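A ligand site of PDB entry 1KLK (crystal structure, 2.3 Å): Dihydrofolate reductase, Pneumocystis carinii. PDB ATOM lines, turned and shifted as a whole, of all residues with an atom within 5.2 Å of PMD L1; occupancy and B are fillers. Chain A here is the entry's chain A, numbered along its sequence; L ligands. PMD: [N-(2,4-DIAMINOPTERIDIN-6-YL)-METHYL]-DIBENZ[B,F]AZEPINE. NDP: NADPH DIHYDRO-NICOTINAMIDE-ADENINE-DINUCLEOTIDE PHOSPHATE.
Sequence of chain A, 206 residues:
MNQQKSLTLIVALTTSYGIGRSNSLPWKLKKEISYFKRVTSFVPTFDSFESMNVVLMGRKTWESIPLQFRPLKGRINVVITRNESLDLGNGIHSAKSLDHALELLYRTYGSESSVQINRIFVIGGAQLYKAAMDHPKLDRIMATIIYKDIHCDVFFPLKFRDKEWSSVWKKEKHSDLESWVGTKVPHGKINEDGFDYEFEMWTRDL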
ATOM      1  N   ILE A  10      18.749   0.787  16.220  1.00  0.00           N
ATOM      2  CA  ILE A  10      18.844   1.329  14.880  1.00  0.00           C
ATOM      3  C   ILE A  10      20.041   0.696  14.184  1.00  0.00           C
ATOM      4  O   ILE A  10      21.158   0.667  14.713  1.00  0.00           O
ATOM      5  CB  ILE A  10      18.945   2.889  14.916  1.00  0.00           C
ATOM      6  CG1 ILE A  10      18.929   3.451  13.492  1.00  0.00           C
ATOM      7  CG2 ILE A  10      20.199   3.344  15.666  1.00  0.00           C
ATOM      8  CD1 ILE A  10      18.787   4.971  13.431  1.00  0.00           C
ATOM      9  N   VAL A  11      19.782   0.159  12.996  1.00  0.00           N
ATOM     10  CA  VAL A  11      20.807  -0.508  12.215  1.00  0.00           C
ATOM     11  C   VAL A  11      20.615  -0.433  10.681  1.00  0.00           C
ATOM     12  O   VAL A  11      19.503  -0.241  10.176  1.00  0.00           O
ATOM     13  CB  VAL A  11      20.903  -1.996  12.662  1.00  0.00           C
ATOM     14  CG1 VAL A  11      19.707  -2.774  12.146  1.00  0.00           C
ATOM     15  CG2 VAL A  11      22.202  -2.605  12.193  1.00  0.00           C
ATOM     16  N   ALA A  12      21.726  -0.518   9.958  1.00  0.00           N
ATOM     17  CA  ALA A  12      21.742  -0.515   8.492  1.00  0.00           C
ATOM     18  C   ALA A  12      22.387  -1.869   8.210  1.00  0.00           C
ATOM     19  O   ALA A  12      23.506  -2.119   8.671  1.00  0.00           O
ATOM     20  CB  ALA A  12      22.639   0.595   7.971  1.00  0.00           C
ATOM     21  N   ASN A  23      36.014  -3.466  10.830  1.00  0.00           N
ATOM     22  CA  ASN A  23      35.747  -2.352  11.734  1.00  0.00           C
ATOM     23  C   ASN A  23      35.407  -1.045  10.997  1.00  0.00           C
ATOM     24  O   ASN A  23      35.786   0.045  11.425  1.00  0.00           O
ATOM     25  CB  ASN A  23      36.961  -2.133  12.650  1.00  0.00           C
ATOM     26  CG  ASN A  23      37.168  -3.273  13.619  1.00  0.00           C
ATOM     27  OD1 ASN A  23      38.135  -3.279  14.375  1.00  0.00           O
ATOM     28  ND2 ASN A  23      36.271  -4.241  13.605  1.00  0.00           N
ATOM     29  N   SER A  24      34.686  -1.179   9.883  1.00  0.00           N
ATOM     30  CA  SER A  24      34.294  -0.025   9.088  1.00  0.00           C
ATOM     31  C   SER A  24      33.017  -0.373   8.309  1.00  0.00           C
ATOM     32  O   SER A  24      32.458  -1.463   8.470  1.00  0.00           O
ATOM     33  CB  SER A  24      35.428   0.352   8.133  1.00  0.00           C
ATOM     34  OG  SER A  24      35.188   1.596   7.487  1.00  0.00           O
ATOM     35  N   LEU A  25      32.545   0.559   7.486  1.00  0.00           N
ATOM     36  CA  LEU A  25      31.341   0.309   6.700  1.00  0.00           C
ATOM     37  C   LEU A  25      31.653   0.151   5.222  1.00  0.00           C
ATOM     38  O   LEU A  25      32.136   1.079   4.575  1.00  0.00           O
ATOM     39  CB  LEU A  25      30.332   1.442   6.879  1.00  0.00           C
ATOM     40  CG  LEU A  25      29.586   1.427   8.209  1.00  0.00           C
ATOM     41  CD1 LEU A  25      28.565   2.530   8.170  1.00  0.00           C
ATOM     42  CD2 LEU A  25      28.909   0.071   8.439  1.00  0.00           C
ATOM     43  N   GLU A  32      21.530   7.974   3.982  1.00  0.00           N
ATOM     44  CA  GLU A  32      21.237   7.111   5.120  1.00  0.00           C
ATOM     45  C   GLU A  32      21.726   7.816   6.369  1.00  0.00           C
ATOM     46  O   GLU A  32      21.036   7.906   7.376  1.00  0.00           O
ATOM     47  CB  GLU A  32      21.962   5.771   4.968  1.00  0.00           C
ATOM     48  CG  GLU A  32      21.290   4.580   5.644  1.00  0.00           C
ATOM     49  CD  GLU A  32      21.279   4.639   7.159  1.00  0.00           C
ATOM     50  OE1 GLU A  32      22.336   4.934   7.749  1.00  0.00           O
ATOM     51  OE2 GLU A  32      20.222   4.378   7.761  1.00  0.00           O
ATOM     52  N   ILE A  33      22.943   8.331   6.296  1.00  0.00           N
ATOM     53  CA  ILE A  33      23.506   9.023   7.440  1.00  0.00           C
ATOM     54  C   ILE A  33      22.628  10.196   7.912  1.00  0.00           C
ATOM     55  O   ILE A  33      22.635  10.517   9.103  1.00  0.00           O
ATOM     56  CB  ILE A  33      24.936   9.519   7.131  1.00  0.00           C
ATOM     57  CG1 ILE A  33      25.849   8.294   6.955  1.00  0.00           C
ATOM     58  CG2 ILE A  33      25.474  10.392   8.277  1.00  0.00           C
ATOM     59  CD1 ILE A  33      25.834   7.341   8.175  1.00  0.00           C
ATOM     60  N   TYR A  35      19.391  10.206   7.705  1.00  0.00           N
ATOM     61  CA  TYR A  35      18.280   9.572   8.373  1.00  0.00           C
ATOM     62  C   TYR A  35      18.720   9.256   9.804  1.00  0.00           C
ATOM     63  O   TYR A  35      18.063   9.637  10.767  1.00  0.00           O
ATOM     64  CB  TYR A  35      17.907   8.286   7.628  1.00  0.00           C
ATOM     65  CG  TYR A  35      16.806   7.497   8.284  1.00  0.00           C
ATOM     66  CD1 TYR A  35      15.505   7.964   8.305  1.00  0.00           C
ATOM     67  CD2 TYR A  35      17.088   6.250   8.873  1.00  0.00           C
ATOM     68  CE1 TYR A  35      14.499   7.239   8.887  1.00  0.00           C
ATOM     69  CE2 TYR A  35      16.085   5.508   9.463  1.00  0.00           C
ATOM     70  CZ  TYR A  35      14.787   6.009   9.462  1.00  0.00           C
ATOM     71  OH  TYR A  35      13.783   5.275  10.048  1.00  0.00           O
ATOM     72  N   PHE A  36      19.837   8.551   9.919  1.00  0.00           N
ATOM     73  CA  PHE A  36      20.367   8.165  11.219  1.00  0.00           C
ATOM     74  C   PHE A  36      20.344   9.318  12.219  1.00  0.00           C
ATOM     75  O   PHE A  36      19.767   9.205  13.307  1.00  0.00           O
ATOM     76  CB  PHE A  36      21.808   7.691  11.068  1.00  0.00           C
ATOM     77  CG  PHE A  36      22.482   7.376  12.380  1.00  0.00           C
ATOM     78  CD1 PHE A  36      22.131   6.243  13.101  1.00  0.00           C
ATOM     79  CD2 PHE A  36      23.422   8.246  12.917  1.00  0.00           C
ATOM     80  CE1 PHE A  36      22.695   6.002  14.346  1.00  0.00           C
ATOM     81  CE2 PHE A  36      23.995   8.005  14.158  1.00  0.00           C
ATOM     82  CZ  PHE A  36      23.630   6.876  14.870  1.00  0.00           C
ATOM     83  N   SER A  64      35.861   3.333  16.171  1.00  0.00           N
ATOM     84  CA  SER A  64      35.831   3.348  14.696  1.00  0.00           C
ATOM     85  C   SER A  64      35.240   4.616  14.096  1.00  0.00           C
ATOM     86  O   SER A  64      35.273   4.811  12.873  1.00  0.00           O
ATOM     87  CB  SER A  64      35.033   2.144  14.164  1.00  0.00           C
ATOM     88  OG  SER A  64      35.621   0.920  14.572  1.00  0.00           O
ATOM     89  N   ILE A  65      34.704   5.479  14.945  1.00  0.00           N
ATOM     90  CA  ILE A  65      34.120   6.735  14.490  1.00  0.00           C
ATOM     91  C   ILE A  65      35.221   7.795  14.497  1.00  0.00           C
ATOM     92  O   ILE A  65      35.781   8.125  15.546  1.00  0.00           O
ATOM     93  CB  ILE A  65      32.981   7.181  15.439  1.00  0.00           C
ATOM     94  CG1 ILE A  65      31.917   6.085  15.525  1.00  0.00           C
ATOM     95  CG2 ILE A  65      32.372   8.489  14.939  1.00  0.00           C
ATOM     96  CD1 ILE A  65      30.774   6.429  16.437  1.00  0.00           C
ATOM     97  N   PRO A  66      35.559   8.350  13.309  1.00  0.00           N
ATOM     98  CA  PRO A  66      36.600   9.378  13.187  1.00  0.00           C
ATOM     99  C   PRO A  66      36.386  10.542  14.149  1.00  0.00           C
ATOM    100  O   PRO A  66      35.298  11.106  14.233  1.00  0.00           O
ATOM    101  CB  PRO A  66      36.504   9.788  11.718  1.00  0.00           C
ATOM    102  CG  PRO A  66      35.074   9.497  11.351  1.00  0.00           C
ATOM    103  CD  PRO A  66      34.862   8.155  12.015  1.00  0.00           C
ATOM    104  N   PHE A  69      34.019  13.188  13.823  1.00  0.00           N
ATOM    105  CA  PHE A  69      32.600  12.909  13.979  1.00  0.00           C
ATOM    106  C   PHE A  69      32.184  12.790  15.437  1.00  0.00           C
ATOM    107  O   PHE A  69      31.479  13.653  15.949  1.00  0.00           O
ATOM    108  CB  PHE A  69      32.235  11.631  13.225  1.00  0.00           C
ATOM    109  CG  PHE A  69      31.357  11.894  12.036  1.00  0.00           C
ATOM    110  CD1 PHE A  69      31.849  12.588  10.939  1.00  0.00           C
ATOM    111  CD2 PHE A  69      30.027  11.479  12.027  1.00  0.00           C
ATOM    112  CE1 PHE A  69      31.026  12.886   9.841  1.00  0.00           C
ATOM    113  CE2 PHE A  69      29.192  11.766  10.954  1.00  0.00           C
ATOM    114  CZ  PHE A  69      29.695  12.473   9.857  1.00  0.00           C
ATOM    115  N   LEU A  72      28.640  11.955  19.086  1.00  0.00           N
ATOM    116  CA  LEU A  72      27.448  12.369  18.396  1.00  0.00           C
ATOM    117  C   LEU A  72      26.789  13.516  19.144  1.00  0.00           C
ATOM    118  O   LEU A  72      26.312  13.358  20.273  1.00  0.00           O
ATOM    119  CB  LEU A  72      26.499  11.178  18.239  1.00  0.00           C
ATOM    120  CG  LEU A  72      27.164   9.960  17.570  1.00  0.00           C
ATOM    121  CD1 LEU A  72      26.096   8.937  17.204  1.00  0.00           C
ATOM    122  CD2 LEU A  72      27.930  10.408  16.334  1.00  0.00           C
ATOM    123  N   ILE A 123      22.815   2.239  19.121  1.00  0.00           N
ATOM    124  CA  ILE A 123      23.331   2.453  17.771  1.00  0.00           C
ATOM    125  C   ILE A 123      24.260   1.402  17.237  1.00  0.00           C
ATOM    126  O   ILE A 123      24.972   1.627  16.255  1.00  0.00           O
ATOM    127  CB  ILE A 123      24.013   3.811  17.627  1.00  0.00           C
ATOM    128  CG1 ILE A 123      25.306   3.836  18.444  1.00  0.00           C
ATOM    129  CG2 ILE A 123      23.051   4.907  18.023  1.00  0.00           C
ATOM    130  CD1 ILE A 123      26.224   4.999  18.033  1.00  0.00           C
ATOM    131  N   GLY A 124      24.299   0.251  17.850  1.00  0.00           N
ATOM    132  CA  GLY A 124      25.158  -0.723  17.264  1.00  0.00           C
ATOM    133  C   GLY A 124      26.398  -1.232  17.913  1.00  0.00           C
ATOM    134  O   GLY A 124      26.921  -0.767  18.948  1.00  0.00           O
ATOM    135  N   TYR A 129      24.339  -5.452  20.027  1.00  0.00           N
ATOM    136  CA  TYR A 129      23.045  -5.731  19.419  1.00  0.00           C
ATOM    137  C   TYR A 129      22.416  -6.949  20.076  1.00  0.00           C
ATOM    138  O   TYR A 129      21.271  -6.892  20.527  1.00  0.00           O
ATOM    139  CB  TYR A 129      23.182  -5.996  17.916  1.00  0.00           C
ATOM    140  CG  TYR A 129      23.227  -4.741  17.095  1.00  0.00           C
ATOM    141  CD1 TYR A 129      22.400  -3.652  17.401  1.00  0.00           C
ATOM    142  CD2 TYR A 129      24.067  -4.639  15.984  1.00  0.00           C
ATOM    143  CE1 TYR A 129      22.422  -2.490  16.623  1.00  0.00           C
ATOM    144  CE2 TYR A 129      24.094  -3.483  15.194  1.00  0.00           C
ATOM    145  CZ  TYR A 129      23.275  -2.415  15.523  1.00  0.00           C
ATOM    146  OH  TYR A 129      23.311  -1.258  14.754  1.00  0.00           O
ATOM    147  N   MET A 142      14.701   0.171  14.086  1.00  0.00           N
ATOM    148  CA  MET A 142      14.732   1.032  12.926  1.00  0.00           C
ATOM    149  C   MET A 142      15.792   0.402  12.016  1.00  0.00           C
ATOM    150  O   MET A 142      16.976   0.406  12.338  1.00  0.00           O
ATOM    151  CB  MET A 142      15.136   2.440  13.363  1.00  0.00           C
ATOM    152  CG  MET A 142      14.181   3.075  14.359  1.00  0.00           C
ATOM    153  SD  MET A 142      12.622   3.566  13.588  1.00  0.00           S
ATOM    154  CE  MET A 142      11.559   2.573  14.427  1.00  0.00           C
ATOM    155  N   THR A 144      17.564  -0.225   8.024  1.00  0.00           N
ATOM    156  CA  THR A 144      17.837   0.268   6.676  1.00  0.00           C
ATOM    157  C   THR A 144      18.364  -0.968   5.946  1.00  0.00           C
ATOM    158  O   THR A 144      19.407  -1.502   6.326  1.00  0.00           O
ATOM    159  CB  THR A 144      18.921   1.349   6.641  1.00  0.00           C
ATOM    160  OG1 THR A 144      18.473   2.531   7.338  1.00  0.00           O
ATOM    161  CG2 THR A 144      19.261   1.699   5.206  1.00  0.00           C
HETATM  162  C2B PMD L   1      21.781   3.363  10.887  1.00  0.00           C
HETATM  163  C4B PMD L   1      23.313   2.542  12.551  1.00  0.00           C
HETATM  164  C4  PMD L   1      24.412   3.063  11.806  1.00  0.00           C
HETATM  165  C6B PMD L   1      26.755   3.440  11.431  1.00  0.00           C
HETATM  166  C7B PMD L   1      26.430   4.124  10.202  1.00  0.00           C
HETATM  167  C8  PMD L   1      24.102   3.740  10.561  1.00  0.00           C
HETATM  168  C9B PMD L   1      28.277   3.272  11.817  1.00  0.00           C
HETATM  169  C0' PMD L   1      30.562   4.020  11.422  1.00  0.00           C
HETATM  170  C1' PMD L   1      30.863   2.651  11.783  1.00  0.00           C
HETATM  171  C2' PMD L   1      32.146   2.105  11.538  1.00  0.00           C
HETATM  172  C3' PMD L   1      33.126   2.881  10.887  1.00  0.00           C
HETATM  173  C4' PMD L   1      32.844   4.215  10.501  1.00  0.00           C
HETATM  174  C5' PMD L   1      31.604   4.843  10.801  1.00  0.00           C
HETATM  175  C6' PMD L   1      31.438   6.280  10.279  1.00  0.00           C
HETATM  176  C6  PMD L   1      30.516   7.211  10.655  1.00  0.00           C
HETATM  177  C7' PMD L   1      29.407   7.054  11.692  1.00  0.00           C
HETATM  178  C8' PMD L   1      28.821   8.279  12.165  1.00  0.00           C
HETATM  179  C9' PMD L   1      27.759   8.279  13.120  1.00  0.00           C
HETATM  180  CA' PMD L   1      27.233   7.055  13.614  1.00  0.00           C
HETATM  181  CB' PMD L   1      27.725   5.830  13.100  1.00  0.00           C
HETATM  182  CC' PMD L   1      28.811   5.782  12.137  1.00  0.00           C
HETATM  183  N1' PMD L   1      22.808   3.881  10.153  1.00  0.00           N
HETATM  184  N2' PMD L   1      20.508   3.480  10.432  1.00  0.00           N
HETATM  185  N3' PMD L   1      22.042   2.711  12.064  1.00  0.00           N
HETATM  186  N4' PMD L   1      23.525   1.889  13.716  1.00  0.00           N
HETATM  187  N5' PMD L   1      25.746   2.924  12.206  1.00  0.00           N
HETATM  188  N8' PMD L   1      25.120   4.258   9.807  1.00  0.00           N
HETATM  189  N0' PMD L   1      29.171   4.486  11.464  1.00  0.00           N
HETATM  190  PA  NDP L   2      30.462  -3.578  19.438  1.00  0.00           P
HETATM  191  O1A NDP L   2      29.856  -2.233  19.360  1.00  0.00           O
HETATM  192  O2A NDP L   2      29.532  -4.692  19.709  1.00  0.00           O
HETATM  193  O5B NDP L   2      31.503  -3.471  20.612  1.00  0.00           O
HETATM  194  C5B NDP L   2      31.835  -4.619  21.369  1.00  0.00           C
HETATM  195  C4B NDP L   2      32.681  -4.127  22.455  1.00  0.00           C
HETATM  196  O4B NDP L   2      31.666  -3.339  23.181  1.00  0.00           O
HETATM  197  C3B NDP L   2      33.184  -5.189  23.431  1.00  0.00           C
HETATM  198  O3B NDP L   2      34.581  -5.567  23.256  1.00  0.00           O
HETATM  199  C2B NDP L   2      32.846  -4.500  24.773  1.00  0.00           C
HETATM  200  O2B NDP L   2      33.835  -4.078  25.779  1.00  0.00           O
HETATM  201  C1B NDP L   2      31.541  -3.817  24.561  1.00  0.00           C
HETATM  202  N9A NDP L   2      30.283  -4.669  24.722  1.00  0.00           N
HETATM  203  C8A NDP L   2      29.543  -5.238  23.719  1.00  0.00           C
HETATM  204  N7A NDP L   2      28.501  -5.929  24.183  1.00  0.00           N
HETATM  205  C5A NDP L   2      28.607  -5.804  25.497  1.00  0.00           C
HETATM  206  C6A NDP L   2      27.713  -6.369  26.447  1.00  0.00           C
HETATM  207  N6A NDP L   2      26.675  -7.105  26.030  1.00  0.00           N
HETATM  208  N1A NDP L   2      27.966  -6.125  27.792  1.00  0.00           N
HETATM  209  C2A NDP L   2      29.038  -5.368  28.154  1.00  0.00           C
HETATM  210  N3A NDP L   2      29.889  -4.824  27.238  1.00  0.00           N
HETATM  211  C4A NDP L   2      29.712  -5.029  25.882  1.00  0.00           C
HETATM  212  O3  NDP L   2      31.222  -3.842  18.056  1.00  0.00           O
HETATM  213  PN  NDP L   2      31.702  -5.234  17.407  1.00  0.00           P
HETATM  214  O1N NDP L   2      30.533  -6.102  17.098  1.00  0.00           O
HETATM  215  O2N NDP L   2      32.791  -5.852  18.212  1.00  0.00           O
HETATM  216  O5D NDP L   2      32.315  -4.758  15.988  1.00  0.00           O
HETATM  217  C5D NDP L   2      32.313  -3.401  15.510  1.00  0.00           C
HETATM  218  C4D NDP L   2      31.657  -3.529  14.118  1.00  0.00           C
HETATM  219  O4D NDP L   2      30.218  -3.219  14.139  1.00  0.00           O
HETATM  220  C3D NDP L   2      32.271  -2.599  13.045  1.00  0.00           C
HETATM  221  O3D NDP L   2      32.429  -3.220  11.726  1.00  0.00           O
HETATM  222  C2D NDP L   2      31.290  -1.453  13.011  1.00  0.00           C
HETATM  223  O2D NDP L   2      31.372  -0.629  11.874  1.00  0.00           O
HETATM  224  C1D NDP L   2      30.007  -2.256  13.077  1.00  0.00           C
HETATM  225  N1N NDP L   2      28.740  -1.461  13.250  1.00  0.00           N
HETATM  226  C2N NDP L   2      27.796  -1.415  12.162  1.00  0.00           C
HETATM  227  C3N NDP L   2      26.577  -0.677  12.282  1.00  0.00           C
HETATM  228  C7N NDP L   2      25.502  -0.593  11.109  1.00  0.00           C
HETATM  229  O7N NDP L   2      24.344  -0.246  11.337  1.00  0.00           O
HETATM  230  N7N NDP L   2      25.893  -0.926   9.879  1.00  0.00           N
HETATM  231  C4N NDP L   2      26.342   0.010  13.510  1.00  0.00           C
HETATM  232  C5N NDP L   2      27.290  -0.042  14.585  1.00  0.00           C
HETATM  233  C6N NDP L   2      28.496  -0.775  14.457  1.00  0.00           C
HETATM  234  P2B NDP L   2      35.369  -4.520  25.830  1.00  0.00           P
HETATM  235  O1X NDP L   2      35.417  -6.012  25.946  1.00  0.00           O
HETATM  236  O2X NDP L   2      36.007  -3.889  27.012  1.00  0.00           O
HETATM  237  O3X NDP L   2      36.075  -4.060  24.630  1.00  0.00           O
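Residues that only touch PMD L1: Leu 25, Phe 36, Phe 69, Ser 64, Val 11, Ile 33, Ser 24, Thr 144, Leu 72, Ala 12 and Asn 23. Hydrophobic or aromatic side chains that line PMD L1: Ile 10, Ala 12, Leu 25, Ile 33, Phe 36, Phe 69 and Leu 72. 15 residues have an atom within 4 Å of PMD L1: Ile 10, Val 11, Ala 12, Asn 23, Ser 24, Leu 25, Glu 32, Ile 33, Phe 36, Ser 64, Phe 69, Leu 72, Ile 123, Tyr 129 and Thr 144. The nearest printed residue that does not touch PMD L1 is Pro 66 (4.3 Å).
OG1 of Thr 144 sits at hydrogen-bond distance from OE2 of Glu 32, 2.6 Å away. The backbone carbonyl oxygen (O) of Ile 10 lies within hydrogen-bond range of the side-chain hydroxyl (OH) of Tyr 129 (2.9 Å). O of Asn 23 lies within hydrogen-bond range of OG of Ser 64. The backbone carbonyl oxygen (O) of Val 11 is in hydrogen-bond range of the backbone NH (N) of Thr 144 (2.9 Å). O of Met 142 is in hydrogen-bond range of N of Val 11 (2.9 Å).
The side-chain carboxylate of Glu 32 sits at hydrogen-bond distance from a nitrogen (N1') of PMD L1. A nitrogen (N4') of PMD L1 lies within hydrogen-bond range of the backbone carbonyl oxygen of Ile 10, 2.8 Å away. O of Ile 123 lies within hydrogen-bond range of N4' of PMD L1, at 2.9 Å. A nitrogen (N4') of PMD L1 is in hydrogen-bond range of the side-chain hydroxyl (OH) of Tyr 129, 3.3 Å away. N of Ala 12 is in hydrogen-bond range of O7N of NDP L2 (3.0 Å). A nitrogen (N7N) of NDP L2 sits at hydrogen-bond distance from the backbone carbonyl oxygen (O) of Ala 12.
O7N of NDP L2 sits close to N4' of PMD L1, 3.3 Å away.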
